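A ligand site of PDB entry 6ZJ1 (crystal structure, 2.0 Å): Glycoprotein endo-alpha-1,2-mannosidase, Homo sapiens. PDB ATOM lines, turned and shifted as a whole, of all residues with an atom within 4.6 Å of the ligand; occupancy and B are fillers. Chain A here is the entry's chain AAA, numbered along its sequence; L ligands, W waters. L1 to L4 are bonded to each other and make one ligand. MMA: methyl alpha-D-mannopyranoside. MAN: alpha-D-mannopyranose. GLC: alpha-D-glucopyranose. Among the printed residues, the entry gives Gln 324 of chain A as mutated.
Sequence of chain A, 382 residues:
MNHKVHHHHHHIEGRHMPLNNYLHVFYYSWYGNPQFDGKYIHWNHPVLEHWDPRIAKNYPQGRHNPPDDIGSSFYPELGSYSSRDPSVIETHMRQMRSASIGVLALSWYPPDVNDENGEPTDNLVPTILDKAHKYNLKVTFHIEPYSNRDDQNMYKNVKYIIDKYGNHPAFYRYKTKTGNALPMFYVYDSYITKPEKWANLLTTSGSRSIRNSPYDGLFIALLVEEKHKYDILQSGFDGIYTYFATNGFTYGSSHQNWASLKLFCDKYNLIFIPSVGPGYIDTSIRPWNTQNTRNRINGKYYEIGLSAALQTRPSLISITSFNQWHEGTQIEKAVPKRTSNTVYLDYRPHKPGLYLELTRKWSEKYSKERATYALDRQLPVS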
ATOM      1  N   TYR A  28      15.688 -16.876   8.913  1.00  0.00           N
ATOM      2  CA  TYR A  28      14.835 -17.823   9.674  1.00  0.00           C
ATOM      3  C   TYR A  28      14.017 -17.030  10.705  1.00  0.00           C
ATOM      4  O   TYR A  28      14.587 -16.181  11.413  1.00  0.00           O
ATOM      5  CB  TYR A  28      15.718 -18.944  10.247  1.00  0.00           C
ATOM      6  CG  TYR A  28      16.426 -19.741   9.173  1.00  0.00           C
ATOM      7  CD1 TYR A  28      17.594 -19.268   8.596  1.00  0.00           C
ATOM      8  CD2 TYR A  28      15.911 -20.940   8.710  1.00  0.00           C
ATOM      9  CE1 TYR A  28      18.232 -19.967   7.594  1.00  0.00           C
ATOM     10  CE2 TYR A  28      16.545 -21.652   7.708  1.00  0.00           C
ATOM     11  CZ  TYR A  28      17.701 -21.152   7.135  1.00  0.00           C
ATOM     12  OH  TYR A  28      18.335 -21.827   6.132  1.00  0.00           O
ATOM     13  N   TRP A  30      12.054 -18.697  13.106  1.00  0.00           N
ATOM     14  CA  TRP A  30      11.616 -19.886  13.896  1.00  0.00           C
ATOM     15  C   TRP A  30      12.098 -19.811  15.353  1.00  0.00           C
ATOM     16  O   TRP A  30      11.744 -20.705  16.091  1.00  0.00           O
ATOM     17  CB  TRP A  30      12.035 -21.208  13.243  1.00  0.00           C
ATOM     18  CG  TRP A  30      13.505 -21.428  13.060  1.00  0.00           C
ATOM     19  CD1 TRP A  30      14.538 -20.784  13.691  1.00  0.00           C
ATOM     20  CD2 TRP A  30      14.131 -22.406  12.205  1.00  0.00           C
ATOM     21  NE1 TRP A  30      15.736 -21.259  13.252  1.00  0.00           N
ATOM     22  CE2 TRP A  30      15.534 -22.265  12.358  1.00  0.00           C
ATOM     23  CE3 TRP A  30      13.661 -23.376  11.325  1.00  0.00           C
ATOM     24  CZ2 TRP A  30      16.448 -23.035  11.646  1.00  0.00           C
ATOM     25  CZ3 TRP A  30      14.572 -24.137  10.624  1.00  0.00           C
ATOM     26  CH2 TRP A  30      15.934 -23.975  10.778  1.00  0.00           C
ATOM     27  N   HIS A  42      13.496 -23.385  19.289  1.00  0.00           N
ATOM     28  CA  HIS A  42      14.771 -23.464  18.517  1.00  0.00           C
ATOM     29  C   HIS A  42      15.979 -23.244  19.414  1.00  0.00           C
ATOM     30  O   HIS A  42      16.878 -24.055  19.264  1.00  0.00           O
ATOM     31  CB  HIS A  42      14.768 -22.583  17.255  1.00  0.00           C
ATOM     32  CG  HIS A  42      14.314 -23.369  16.084  1.00  0.00           C
ATOM     33  ND1 HIS A  42      15.161 -24.183  15.387  1.00  0.00           N
ATOM     34  CD2 HIS A  42      13.069 -23.549  15.560  1.00  0.00           C
ATOM     35  CE1 HIS A  42      14.473 -24.832  14.459  1.00  0.00           C
ATOM     36  NE2 HIS A  42      13.183 -24.463  14.551  1.00  0.00           N
ATOM     37  N   HIS A  45      17.379 -26.187  21.556  1.00  0.00           N
ATOM     38  CA  HIS A  45      17.461 -27.224  20.504  1.00  0.00           C
ATOM     39  C   HIS A  45      17.985 -28.473  21.200  1.00  0.00           C
ATOM     40  O   HIS A  45      18.867 -28.375  22.042  1.00  0.00           O
ATOM     41  CB  HIS A  45      18.334 -26.807  19.323  1.00  0.00           C
ATOM     42  CG  HIS A  45      18.050 -27.501  18.037  1.00  0.00           C
ATOM     43  ND1 HIS A  45      18.542 -28.769  17.729  1.00  0.00           N
ATOM     44  CD2 HIS A  45      17.384 -27.091  16.929  1.00  0.00           C
ATOM     45  CE1 HIS A  45      18.186 -29.101  16.517  1.00  0.00           C
ATOM     46  NE2 HIS A  45      17.487 -28.079  15.990  1.00  0.00           N
ATOM     47  N   TYR A 109       7.277 -22.794   5.664  1.00  0.00           N
ATOM     48  CA  TYR A 109       6.440 -24.021   5.785  1.00  0.00           C
ATOM     49  C   TYR A 109       4.977 -23.650   5.618  1.00  0.00           C
ATOM     50  O   TYR A 109       4.529 -22.582   6.038  1.00  0.00           O
ATOM     51  CB  TYR A 109       6.661 -24.728   7.135  1.00  0.00           C
ATOM     52  CG  TYR A 109       7.940 -25.527   7.239  1.00  0.00           C
ATOM     53  CD1 TYR A 109       9.151 -24.930   7.538  1.00  0.00           C
ATOM     54  CD2 TYR A 109       7.934 -26.912   7.037  1.00  0.00           C
ATOM     55  CE1 TYR A 109      10.311 -25.678   7.657  1.00  0.00           C
ATOM     56  CE2 TYR A 109       9.084 -27.663   7.120  1.00  0.00           C
ATOM     57  CZ  TYR A 109      10.284 -27.054   7.434  1.00  0.00           C
ATOM     58  OH  TYR A 109      11.425 -27.795   7.515  1.00  0.00           O
ATOM     59  N   ASP A 115       9.119 -27.011  10.859  1.00  0.00           N
ATOM     60  CA  ASP A 115      10.321 -27.872  10.973  1.00  0.00           C
ATOM     61  C   ASP A 115      10.140 -28.702  12.242  1.00  0.00           C
ATOM     62  O   ASP A 115       9.478 -28.203  13.198  1.00  0.00           O
ATOM     63  CB  ASP A 115      11.624 -27.060  11.029  1.00  0.00           C
ATOM     64  CG  ASP A 115      11.981 -26.507  12.402  1.00  0.00           C
ATOM     65  OD1 ASP A 115      11.373 -25.471  12.815  1.00  0.00           O
ATOM     66  OD2 ASP A 115      12.869 -27.098  13.062  1.00  0.00           O
ATOM     67  N   GLU A 116      10.791 -29.865  12.271  1.00  0.00           N
ATOM     68  CA  GLU A 116      10.691 -30.920  13.315  1.00  0.00           C
ATOM     69  C   GLU A 116      11.079 -30.402  14.720  1.00  0.00           C
ATOM     70  O   GLU A 116      10.709 -31.072  15.691  1.00  0.00           O
ATOM     71  CB  GLU A 116      11.536 -32.116  12.844  1.00  0.00           C
ATOM     72  CG  GLU A 116      12.905 -31.767  12.228  1.00  0.00           C
ATOM     73  CD  GLU A 116      13.000 -31.479  10.718  1.00  0.00           C
ATOM     74  OE1 GLU A 116      13.663 -32.256   9.993  1.00  0.00           O
ATOM     75  OE2 GLU A 116      12.463 -30.435  10.268  1.00  0.00           O
ATOM     76  N   ASN A 117      11.807 -29.278  14.826  1.00  0.00           N
ATOM     77  CA  ASN A 117      12.311 -28.686  16.116  1.00  0.00           C
ATOM     78  C   ASN A 117      11.717 -27.288  16.358  1.00  0.00           C
ATOM     79  O   ASN A 117      12.272 -26.550  17.170  1.00  0.00           O
ATOM     80  CB  ASN A 117      13.837 -28.503  16.144  1.00  0.00           C
ATOM     81  CG  ASN A 117      14.611 -29.787  15.916  1.00  0.00           C
ATOM     82  OD1 ASN A 117      14.697 -30.612  16.810  1.00  0.00           O
ATOM     83  ND2 ASN A 117      15.140 -29.989  14.720  1.00  0.00           N
ATOM     84  N   HIS A 142      11.888 -19.233   0.615  1.00  0.00           N
ATOM     85  CA  HIS A 142      12.798 -20.398   0.594  1.00  0.00           C
ATOM     86  C   HIS A 142      11.982 -21.641   0.991  1.00  0.00           C
ATOM     87  O   HIS A 142      11.761 -21.853   2.218  1.00  0.00           O
ATOM     88  CB  HIS A 142      13.991 -20.098   1.499  1.00  0.00           C
ATOM     89  CG  HIS A 142      15.080 -21.109   1.444  1.00  0.00           C
ATOM     90  ND1 HIS A 142      16.069 -21.150   2.388  1.00  0.00           N
ATOM     91  CD2 HIS A 142      15.339 -22.118   0.576  1.00  0.00           C
ATOM     92  CE1 HIS A 142      16.912 -22.117   2.088  1.00  0.00           C
ATOM     93  NE2 HIS A 142      16.490 -22.729   0.994  1.00  0.00           N
ATOM     94  N   GLU A 144      10.989 -24.963   2.099  1.00  0.00           N
ATOM     95  CA  GLU A 144      11.593 -26.071   2.889  1.00  0.00           C
ATOM     96  C   GLU A 144      10.947 -27.375   2.470  1.00  0.00           C
ATOM     97  O   GLU A 144       9.890 -27.356   1.838  1.00  0.00           O
ATOM     98  CB  GLU A 144      11.429 -25.845   4.390  1.00  0.00           C
ATOM     99  CG  GLU A 144      12.224 -24.652   4.928  1.00  0.00           C
ATOM    100  CD  GLU A 144      13.726 -24.848   5.056  1.00  0.00           C
ATOM    101  OE1 GLU A 144      14.187 -25.971   4.795  1.00  0.00           O
ATOM    102  OE2 GLU A 144      14.422 -23.861   5.399  1.00  0.00           O
ATOM    103  N   PRO A 145      11.570 -28.537   2.804  1.00  0.00           N
ATOM    104  CA  PRO A 145      11.041 -29.839   2.439  1.00  0.00           C
ATOM    105  C   PRO A 145       9.944 -30.290   3.420  1.00  0.00           C
ATOM    106  O   PRO A 145      10.214 -31.156   4.220  1.00  0.00           O
ATOM    107  CB  PRO A 145      12.258 -30.781   2.544  1.00  0.00           C
ATOM    108  CG  PRO A 145      13.445 -29.887   2.789  1.00  0.00           C
ATOM    109  CD  PRO A 145      12.874 -28.661   3.466  1.00  0.00           C
ATOM    110  N   TYR A 188      14.264 -25.710  -1.427  1.00  0.00           N
ATOM    111  CA  TYR A 188      15.231 -26.514  -0.627  1.00  0.00           C
ATOM    112  C   TYR A 188      14.976 -28.026  -0.852  1.00  0.00           C
ATOM    113  O   TYR A 188      13.803 -28.512  -0.775  1.00  0.00           O
ATOM    114  CB  TYR A 188      15.254 -26.107   0.859  1.00  0.00           C
ATOM    115  CG  TYR A 188      16.460 -26.708   1.534  1.00  0.00           C
ATOM    116  CD1 TYR A 188      17.734 -26.266   1.219  1.00  0.00           C
ATOM    117  CD2 TYR A 188      16.342 -27.855   2.309  1.00  0.00           C
ATOM    118  CE1 TYR A 188      18.858 -26.908   1.734  1.00  0.00           C
ATOM    119  CE2 TYR A 188      17.447 -28.504   2.815  1.00  0.00           C
ATOM    120  CZ  TYR A 188      18.709 -28.043   2.511  1.00  0.00           C
ATOM    121  OH  TYR A 188      19.798 -28.665   3.038  1.00  0.00           O
ATOM    122  N   ASP A 189      16.049 -28.759  -1.185  1.00  0.00           N
ATOM    123  CA  ASP A 189      16.071 -30.237  -1.366  1.00  0.00           C
ATOM    124  C   ASP A 189      15.110 -30.637  -2.498  1.00  0.00           C
ATOM    125  O   ASP A 189      14.485 -31.722  -2.429  1.00  0.00           O
ATOM    126  CB  ASP A 189      15.806 -30.955  -0.038  1.00  0.00           C
ATOM    127  CG  ASP A 189      17.026 -31.153   0.836  1.00  0.00           C
ATOM    128  OD1 ASP A 189      18.124 -30.720   0.431  1.00  0.00           O
ATOM    129  OD2 ASP A 189      16.881 -31.734   1.914  1.00  0.00           O
ATOM    130  N   TYR A 191      15.795 -32.063  -5.217  1.00  0.00           N
ATOM    131  CA  TYR A 191      16.231 -33.379  -5.781  1.00  0.00           C
ATOM    132  C   TYR A 191      15.419 -34.553  -5.210  1.00  0.00           C
ATOM    133  O   TYR A 191      15.488 -35.646  -5.751  1.00  0.00           O
ATOM    134  CB  TYR A 191      17.748 -33.590  -5.575  1.00  0.00           C
ATOM    135  CG  TYR A 191      18.233 -33.680  -4.138  1.00  0.00           C
ATOM    136  CD1 TYR A 191      18.538 -32.541  -3.396  1.00  0.00           C
ATOM    137  CD2 TYR A 191      18.407 -34.906  -3.519  1.00  0.00           C
ATOM    138  CE1 TYR A 191      18.986 -32.630  -2.086  1.00  0.00           C
ATOM    139  CE2 TYR A 191      18.860 -35.011  -2.214  1.00  0.00           C
ATOM    140  CZ  TYR A 191      19.152 -33.866  -1.497  1.00  0.00           C
ATOM    141  OH  TYR A 191      19.597 -33.960  -0.210  1.00  0.00           O
ATOM    142  N   LEU A 222      17.943 -26.656  -5.763  1.00  0.00           N
ATOM    143  CA  LEU A 222      19.181 -26.901  -5.037  1.00  0.00           C
ATOM    144  C   LEU A 222      19.978 -27.958  -5.800  1.00  0.00           C
ATOM    145  O   LEU A 222      19.479 -29.082  -5.949  1.00  0.00           O
ATOM    146  CB  LEU A 222      18.857 -27.344  -3.622  1.00  0.00           C
ATOM    147  CG  LEU A 222      20.092 -27.532  -2.769  1.00  0.00           C
ATOM    148  CD1 LEU A 222      20.623 -26.188  -2.300  1.00  0.00           C
ATOM    149  CD2 LEU A 222      19.763 -28.419  -1.575  1.00  0.00           C
ATOM    150  N   VAL A 224      23.082 -30.291  -5.499  1.00  0.00           N
ATOM    151  CA  VAL A 224      23.975 -30.961  -4.511  1.00  0.00           C
ATOM    152  C   VAL A 224      25.110 -31.660  -5.257  1.00  0.00           C
ATOM    153  O   VAL A 224      26.276 -31.245  -5.095  1.00  0.00           O
ATOM    154  CB  VAL A 224      23.195 -31.923  -3.614  1.00  0.00           C
ATOM    155  CG1 VAL A 224      24.116 -32.655  -2.646  1.00  0.00           C
ATOM    156  CG2 VAL A 224      22.089 -31.198  -2.854  1.00  0.00           C
ATOM    157  N   TYR A 243      23.272 -23.282  -1.542  1.00  0.00           N
ATOM    158  CA  TYR A 243      22.951 -23.118  -0.088  1.00  0.00           C
ATOM    159  C   TYR A 243      24.144 -23.301   0.876  1.00  0.00           C
ATOM    160  O   TYR A 243      24.469 -22.341   1.593  1.00  0.00           O
ATOM    161  CB  TYR A 243      21.780 -23.999   0.331  1.00  0.00           C
ATOM    162  CG  TYR A 243      21.430 -23.696   1.757  1.00  0.00           C
ATOM    163  CD1 TYR A 243      20.675 -22.580   2.076  1.00  0.00           C
ATOM    164  CD2 TYR A 243      21.974 -24.458   2.779  1.00  0.00           C
ATOM    165  CE1 TYR A 243      20.414 -22.261   3.396  1.00  0.00           C
ATOM    166  CE2 TYR A 243      21.728 -24.144   4.107  1.00  0.00           C
ATOM    167  CZ  TYR A 243      20.953 -23.037   4.418  1.00  0.00           C
ATOM    168  OH  TYR A 243      20.740 -22.734   5.726  1.00  0.00           O
ATOM    169  N   PHE A 244      24.757 -24.490   0.959  1.00  0.00           N
ATOM    170  CA  PHE A 244      25.705 -24.881   2.042  1.00  0.00           C
ATOM    171  C   PHE A 244      26.882 -23.903   2.116  1.00  0.00           C
ATOM    172  O   PHE A 244      27.449 -23.589   1.051  1.00  0.00           O
ATOM    173  CB  PHE A 244      26.185 -26.330   1.863  1.00  0.00           C
ATOM    174  CG  PHE A 244      25.042 -27.254   1.606  1.00  0.00           C
ATOM    175  CD1 PHE A 244      24.146 -27.553   2.614  1.00  0.00           C
ATOM    176  CD2 PHE A 244      24.814 -27.743   0.336  1.00  0.00           C
ATOM    177  CE1 PHE A 244      23.046 -28.357   2.361  1.00  0.00           C
ATOM    178  CE2 PHE A 244      23.709 -28.516   0.075  1.00  0.00           C
ATOM    179  CZ  PHE A 244      22.822 -28.818   1.079  1.00  0.00           C
ATOM    180  N   PHE A 249      31.563 -29.444   1.142  1.00  0.00           N
ATOM    181  CA  PHE A 249      30.485 -30.303   1.712  1.00  0.00           C
ATOM    182  C   PHE A 249      29.783 -31.076   0.605  1.00  0.00           C
ATOM    183  O   PHE A 249      29.554 -32.286   0.809  1.00  0.00           O
ATOM    184  CB  PHE A 249      29.475 -29.477   2.494  1.00  0.00           C
ATOM    185  CG  PHE A 249      28.315 -30.291   3.019  1.00  0.00           C
ATOM    186  CD1 PHE A 249      28.531 -31.430   3.764  1.00  0.00           C
ATOM    187  CD2 PHE A 249      27.005 -29.905   2.753  1.00  0.00           C
ATOM    188  CE1 PHE A 249      27.471 -32.195   4.224  1.00  0.00           C
ATOM    189  CE2 PHE A 249      25.939 -30.675   3.207  1.00  0.00           C
ATOM    190  CZ  PHE A 249      26.173 -31.820   3.942  1.00  0.00           C
ATOM    191  N   THR A 250      29.405 -30.395  -0.479  1.00  0.00           N
ATOM    192  CA  THR A 250      28.767 -30.971  -1.698  1.00  0.00           C
ATOM    193  C   THR A 250      29.505 -30.487  -2.943  1.00  0.00           C
ATOM    194  O   THR A 250      30.349 -29.578  -2.820  1.00  0.00           O
ATOM    195  CB  THR A 250      27.287 -30.588  -1.797  1.00  0.00           C
ATOM    196  OG1 THR A 250      27.158 -29.208  -2.116  1.00  0.00           O
ATOM    197  CG2 THR A 250      26.528 -30.892  -0.529  1.00  0.00           C
ATOM    198  N   TYR A 280      31.036 -22.225   9.156  1.00  0.00           N
ATOM    199  CA  TYR A 280      30.077 -23.267   9.603  1.00  0.00           C
ATOM    200  C   TYR A 280      30.562 -23.822  10.942  1.00  0.00           C
ATOM    201  O   TYR A 280      31.771 -24.031  11.053  1.00  0.00           O
ATOM    202  CB  TYR A 280      29.949 -24.403   8.580  1.00  0.00           C
ATOM    203  CG  TYR A 280      28.758 -25.294   8.806  1.00  0.00           C
ATOM    204  CD1 TYR A 280      27.503 -25.003   8.275  1.00  0.00           C
ATOM    205  CD2 TYR A 280      28.849 -26.419   9.617  1.00  0.00           C
ATOM    206  CE1 TYR A 280      26.397 -25.812   8.515  1.00  0.00           C
ATOM    207  CE2 TYR A 280      27.746 -27.223   9.881  1.00  0.00           C
ATOM    208  CZ  TYR A 280      26.513 -26.925   9.341  1.00  0.00           C
ATOM    209  OH  TYR A 280      25.457 -27.753   9.616  1.00  0.00           O
ATOM    210  N   ILE A 285      24.637 -28.999  18.316  1.00  0.00           N
ATOM    211  CA  ILE A 285      23.450 -29.885  18.065  1.00  0.00           C
ATOM    212  C   ILE A 285      23.785 -31.101  17.162  1.00  0.00           C
ATOM    213  O   ILE A 285      22.910 -31.975  17.006  1.00  0.00           O
ATOM    214  CB  ILE A 285      22.293 -29.048  17.480  1.00  0.00           C
ATOM    215  CG1 ILE A 285      22.669 -28.445  16.121  1.00  0.00           C
ATOM    216  CG2 ILE A 285      21.858 -27.971  18.461  1.00  0.00           C
ATOM    217  CD1 ILE A 285      21.505 -28.377  15.151  1.00  0.00           C
ATOM    218  N   ARG A 286      24.973 -31.169  16.566  1.00  0.00           N
ATOM    219  CA  ARG A 286      25.411 -32.312  15.715  1.00  0.00           C
ATOM    220  C   ARG A 286      26.872 -32.589  16.072  1.00  0.00           C
ATOM    221  O   ARG A 286      27.792 -32.291  15.293  1.00  0.00           O
ATOM    222  CB  ARG A 286      25.270 -32.006  14.223  1.00  0.00           C
ATOM    223  CG  ARG A 286      23.830 -31.882  13.742  1.00  0.00           C
ATOM    224  CD  ARG A 286      23.718 -31.804  12.227  1.00  0.00           C
ATOM    225  NE  ARG A 286      22.372 -31.371  11.829  1.00  0.00           N
ATOM    226  CZ  ARG A 286      22.018 -30.120  11.532  1.00  0.00           C
ATOM    227  NH1 ARG A 286      22.899 -29.138  11.530  1.00  0.00           N
ATOM    228  NH2 ARG A 286      20.757 -29.856  11.216  1.00  0.00           N
ATOM    229  N   ASN A 289      29.604 -33.738  13.726  1.00  0.00           N
ATOM    230  CA  ASN A 289      29.706 -33.074  12.397  1.00  0.00           C
ATOM    231  C   ASN A 289      30.860 -32.070  12.375  1.00  0.00           C
ATOM    232  O   ASN A 289      30.714 -31.006  11.756  1.00  0.00           O
ATOM    233  CB  ASN A 289      28.359 -32.438  12.002  1.00  0.00           C
ATOM    234  CG  ASN A 289      28.267 -32.098  10.533  1.00  0.00           C
ATOM    235  OD1 ASN A 289      28.920 -32.717   9.717  1.00  0.00           O
ATOM    236  ND2 ASN A 289      27.465 -31.096  10.191  1.00  0.00           N
ATOM    237  N   GLN A 324      21.015 -18.311  10.856  1.00  0.00           N
ATOM    238  CA  GLN A 324      21.061 -19.760  11.177  1.00  0.00           C
ATOM    239  C   GLN A 324      22.120 -19.937  12.282  1.00  0.00           C
ATOM    240  O   GLN A 324      23.322 -20.108  11.962  1.00  0.00           O
ATOM    241  CB  GLN A 324      21.337 -20.629   9.943  1.00  0.00           C
ATOM    242  CG  GLN A 324      20.448 -21.869   9.837  1.00  0.00           C
ATOM    243  CD  GLN A 324      20.474 -22.853  10.993  1.00  0.00           C
ATOM    244  OE1 GLN A 324      21.119 -22.644  12.026  1.00  0.00           O
ATOM    245  NE2 GLN A 324      19.765 -23.960  10.825  1.00  0.00           N
ATOM    246  N   HIS A 326      22.236 -22.229  14.840  1.00  0.00           N
ATOM    247  CA  HIS A 326      22.528 -23.667  15.080  1.00  0.00           C
ATOM    248  C   HIS A 326      23.760 -24.091  14.272  1.00  0.00           C
ATOM    249  O   HIS A 326      24.635 -24.757  14.851  1.00  0.00           O
ATOM    250  CB  HIS A 326      21.309 -24.508  14.726  1.00  0.00           C
ATOM    251  CG  HIS A 326      20.014 -24.094  15.346  1.00  0.00           C
ATOM    252  ND1 HIS A 326      19.892 -23.795  16.688  1.00  0.00           N
ATOM    253  CD2 HIS A 326      18.770 -24.025  14.819  1.00  0.00           C
ATOM    254  CE1 HIS A 326      18.628 -23.516  16.941  1.00  0.00           C
ATOM    255  NE2 HIS A 326      17.909 -23.659  15.822  1.00  0.00           N
ATOM    256  N   GLU A 327      23.877 -23.637  13.013  1.00  0.00           N
ATOM    257  CA  GLU A 327      24.929 -24.059  12.062  1.00  0.00           C
ATOM    258  C   GLU A 327      26.091 -23.066  12.058  1.00  0.00           C
ATOM    259  O   GLU A 327      27.107 -23.348  11.398  1.00  0.00           O
ATOM    260  CB  GLU A 327      24.294 -24.307  10.693  1.00  0.00           C
ATOM    261  CG  GLU A 327      23.275 -25.406  10.756  1.00  0.00           C
ATOM    262  CD  GLU A 327      22.705 -25.944   9.445  1.00  0.00           C
ATOM    263  OE1 GLU A 327      22.927 -25.323   8.393  1.00  0.00           O
ATOM    264  OE2 GLU A 327      22.014 -26.981   9.517  1.00  0.00           O
HETATM  265  C1  MMA L   1      22.147 -32.876   4.619  1.00  0.00           C
HETATM  266  C2  MMA L   1      20.943 -31.914   4.672  1.00  0.00           C
HETATM  267  C3  MMA L   1      20.083 -32.122   3.433  1.00  0.00           C
HETATM  268  C4  MMA L   1      20.944 -31.857   2.218  1.00  0.00           C
HETATM  269  C5  MMA L   1      22.098 -32.832   2.170  1.00  0.00           C
HETATM  270  C6  MMA L   1      22.970 -32.518   0.967  1.00  0.00           C
HETATM  271  C7  MMA L   1      22.567 -35.290   4.748  1.00  0.00           C
HETATM  272  O1  MMA L   1      21.637 -34.196   4.861  1.00  0.00           O
HETATM  273  O2  MMA L   1      21.304 -30.497   4.759  1.00  0.00           O
HETATM  274  O3  MMA L   1      18.985 -31.234   3.442  1.00  0.00           O
HETATM  275  O4  MMA L   1      20.176 -31.972   1.041  1.00  0.00           O
HETATM  276  O5  MMA L   1      22.854 -32.788   3.370  1.00  0.00           O
HETATM  277  O6  MMA L   1      23.970 -33.532   0.820  1.00  0.00           O
HETATM  278  C1  MAN L   2      20.755 -29.880   5.924  1.00  0.00           C
HETATM  279  C2  MAN L   2      21.044 -28.361   5.973  1.00  0.00           C
HETATM  280  C3  MAN L   2      22.586 -28.068   6.128  1.00  0.00           C
HETATM  281  C4  MAN L   2      23.215 -28.886   7.249  1.00  0.00           C
HETATM  282  C5  MAN L   2      22.780 -30.343   7.119  1.00  0.00           C
HETATM  283  C6  MAN L   2      23.354 -31.194   8.268  1.00  0.00           C
HETATM  284  O2  MAN L   2      20.114 -27.879   6.955  1.00  0.00           O
HETATM  285  O3  MAN L   2      22.952 -26.652   6.164  1.00  0.00           O
HETATM  286  O4  MAN L   2      24.659 -28.823   7.228  1.00  0.00           O
HETATM  287  O5  MAN L   2      21.350 -30.455   7.090  1.00  0.00           O
HETATM  288  O6  MAN L   2      23.573 -32.509   7.766  1.00  0.00           O
HETATM  289  C1  MAN L   3      19.955 -26.448   7.073  1.00  0.00           C
HETATM  290  C2  MAN L   3      19.029 -26.364   8.259  1.00  0.00           C
HETATM  291  C3  MAN L   3      17.754 -27.138   7.851  1.00  0.00           C
HETATM  292  C4  MAN L   3      17.014 -26.409   6.759  1.00  0.00           C
HETATM  293  C5  MAN L   3      17.998 -26.115   5.615  1.00  0.00           C
HETATM  294  C6  MAN L   3      17.423 -25.066   4.678  1.00  0.00           C
HETATM  295  O2  MAN L   3      18.883 -24.966   8.565  1.00  0.00           O
HETATM  296  O3  MAN L   3      16.815 -27.364   8.929  1.00  0.00           O
HETATM  297  O4  MAN L   3      15.894 -27.217   6.369  1.00  0.00           O
HETATM  298  O5  MAN L   3      19.307 -25.662   6.044  1.00  0.00           O
HETATM  299  O6  MAN L   3      17.018 -23.854   5.317  1.00  0.00           O
HETATM  300  C1  GLC L   4      17.235 -28.503   9.732  1.00  0.00           C
HETATM  301  C2  GLC L   4      15.972 -29.072  10.393  1.00  0.00           C
HETATM  302  C3  GLC L   4      15.614 -28.202  11.588  1.00  0.00           C
HETATM  303  C4  GLC L   4      16.816 -28.019  12.537  1.00  0.00           C
HETATM  304  C5  GLC L   4      18.003 -27.399  11.820  1.00  0.00           C
HETATM  305  C6  GLC L   4      19.265 -27.362  12.667  1.00  0.00           C
HETATM  306  O2  GLC L   4      14.914 -29.170   9.390  1.00  0.00           O
HETATM  307  O3  GLC L   4      14.502 -28.744  12.284  1.00  0.00           O
HETATM  308  O4  GLC L   4      16.423 -27.169  13.560  1.00  0.00           O
HETATM  309  O5  GLC L   4      18.312 -28.161  10.640  1.00  0.00           O
HETATM  310  O6  GLC L   4      20.407 -26.912  11.913  1.00  0.00           O
HETATM  311  O   HOH W   1      25.284 -24.552   5.540  1.00  0.00           O
HETATM  312  O   HOH W   2      13.871 -27.036   8.330  1.00  0.00           O
HETATM  313  O   HOH W   3      23.353 -35.437  -0.733  1.00  0.00           O
HETATM  314  O   HOH W   4      16.322 -30.265   6.473  1.00  0.00           O
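O4 of MMA L1 lies within hydrogen-bond range of OH of Tyr 191, 2.4 Å away.
The side-chain carboxylate (OD2) of Asp 115 sits at hydrogen-bond distance from an oxygen (O3) of GLC L4 (2.4 Å).
The side-chain carboxylate (OD1) of Asp 189 lies within hydrogen-bond range of an oxygen (O4) of MMA L1.
The side-chain hydroxyl of Tyr 28 is in hydrogen-bond range of an oxygen (O6) of MAN L3 (2.6 Å).
O3 of MAN L2 is in hydrogen-bond range of OE1 of Glu 327 (2.6 Å).
An oxygen (O6) of MAN L3 lies within hydrogen-bond range of the side-chain carboxylate of Glu 144 (2.6 Å).
An oxygen (O2) of MAN L3 sits at hydrogen-bond distance from the side-chain amide nitrogen (NE2) of Gln 324.
OH of Tyr 188 lies within hydrogen-bond range of O3 of MMA L1.
O4 of MAN L2 sits at hydrogen-bond distance from OH of Tyr 280.
A ring nitrogen (NE2) of His 45 sits at hydrogen-bond distance from an oxygen (O4) of GLC L4.
An oxygen (O3) of GLC L4 lies within hydrogen-bond range of the side-chain amide nitrogen (ND2) of Asn 117, 2.8 Å away.
An oxygen (O2) of GLC L4 is in hydrogen-bond range of the side-chain carboxylate of Glu 116, at 2.9 Å.
The guanidinium group (NH2) of Arg 286 lies within hydrogen-bond range of an oxygen (O5) of GLC L4.
O5 of MAN L3 sits at hydrogen-bond distance from OH of Tyr 243.
N of Asn 117 is in hydrogen-bond range of OD2 of Asp 115 (3.0 Å).
OD1 of Asp 115 lies within hydrogen-bond range of NE2 of His 42 (2.7 Å).
OH of Tyr 28 lies within hydrogen-bond range of OH of Tyr 243 (2.6 Å).
OE1 of Gln 324 lies within hydrogen-bond range of N of Glu 327 (3.1 Å).
The guanidinium group (NH1) of Arg 286 is in salt-bridge range of the side-chain carboxylate (OE2) of Glu 327 (3.1 Å).
The side-chain amide oxygen (OE1) of Gln 324 sits at hydrogen-bond distance from the backbone NH (N) of His 326, at 3.1 Å.
The side-chain amide nitrogen (ND2) of Asn 117 sits at hydrogen-bond distance from a ring nitrogen (NE2) of His 45, at 3.3 Å.
A ring nitrogen (ND1) of His 42 sits at hydrogen-bond distance from a ring nitrogen (NE2) of His 326, at 2.8 Å.
Water W2 lies within hydrogen-bond range of an oxygen (O2) of GLC L4 and the side-chain hydroxyl of Tyr 109.
Residues that only touch the ligand: Trp 30 (3.8 Å), His 42 (3.2 Å), His 142 (3.7 Å), Val 224 (3.6 Å), Phe 244 (3.7 Å), Phe 249 (3.5 Å), Thr 250 (3.9 Å), Ile 285 (3.5 Å) and His 326 (3.8 Å).
Within 4 Å of the ligand: Tyr 28, Trp 30, His 42, His 45, Asp 115, Glu 116, Asn 117, His 142, Glu 144, Tyr 188, Asp 189, Tyr 191, Val 224, Tyr 243, Phe 244, Phe 249, Thr 250, Tyr 280, Ile 285, Arg 286, Gln 324, His 326 and Glu 327.
Along chain A the residues within 4 Å of the ligand span positions 28 to 327.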
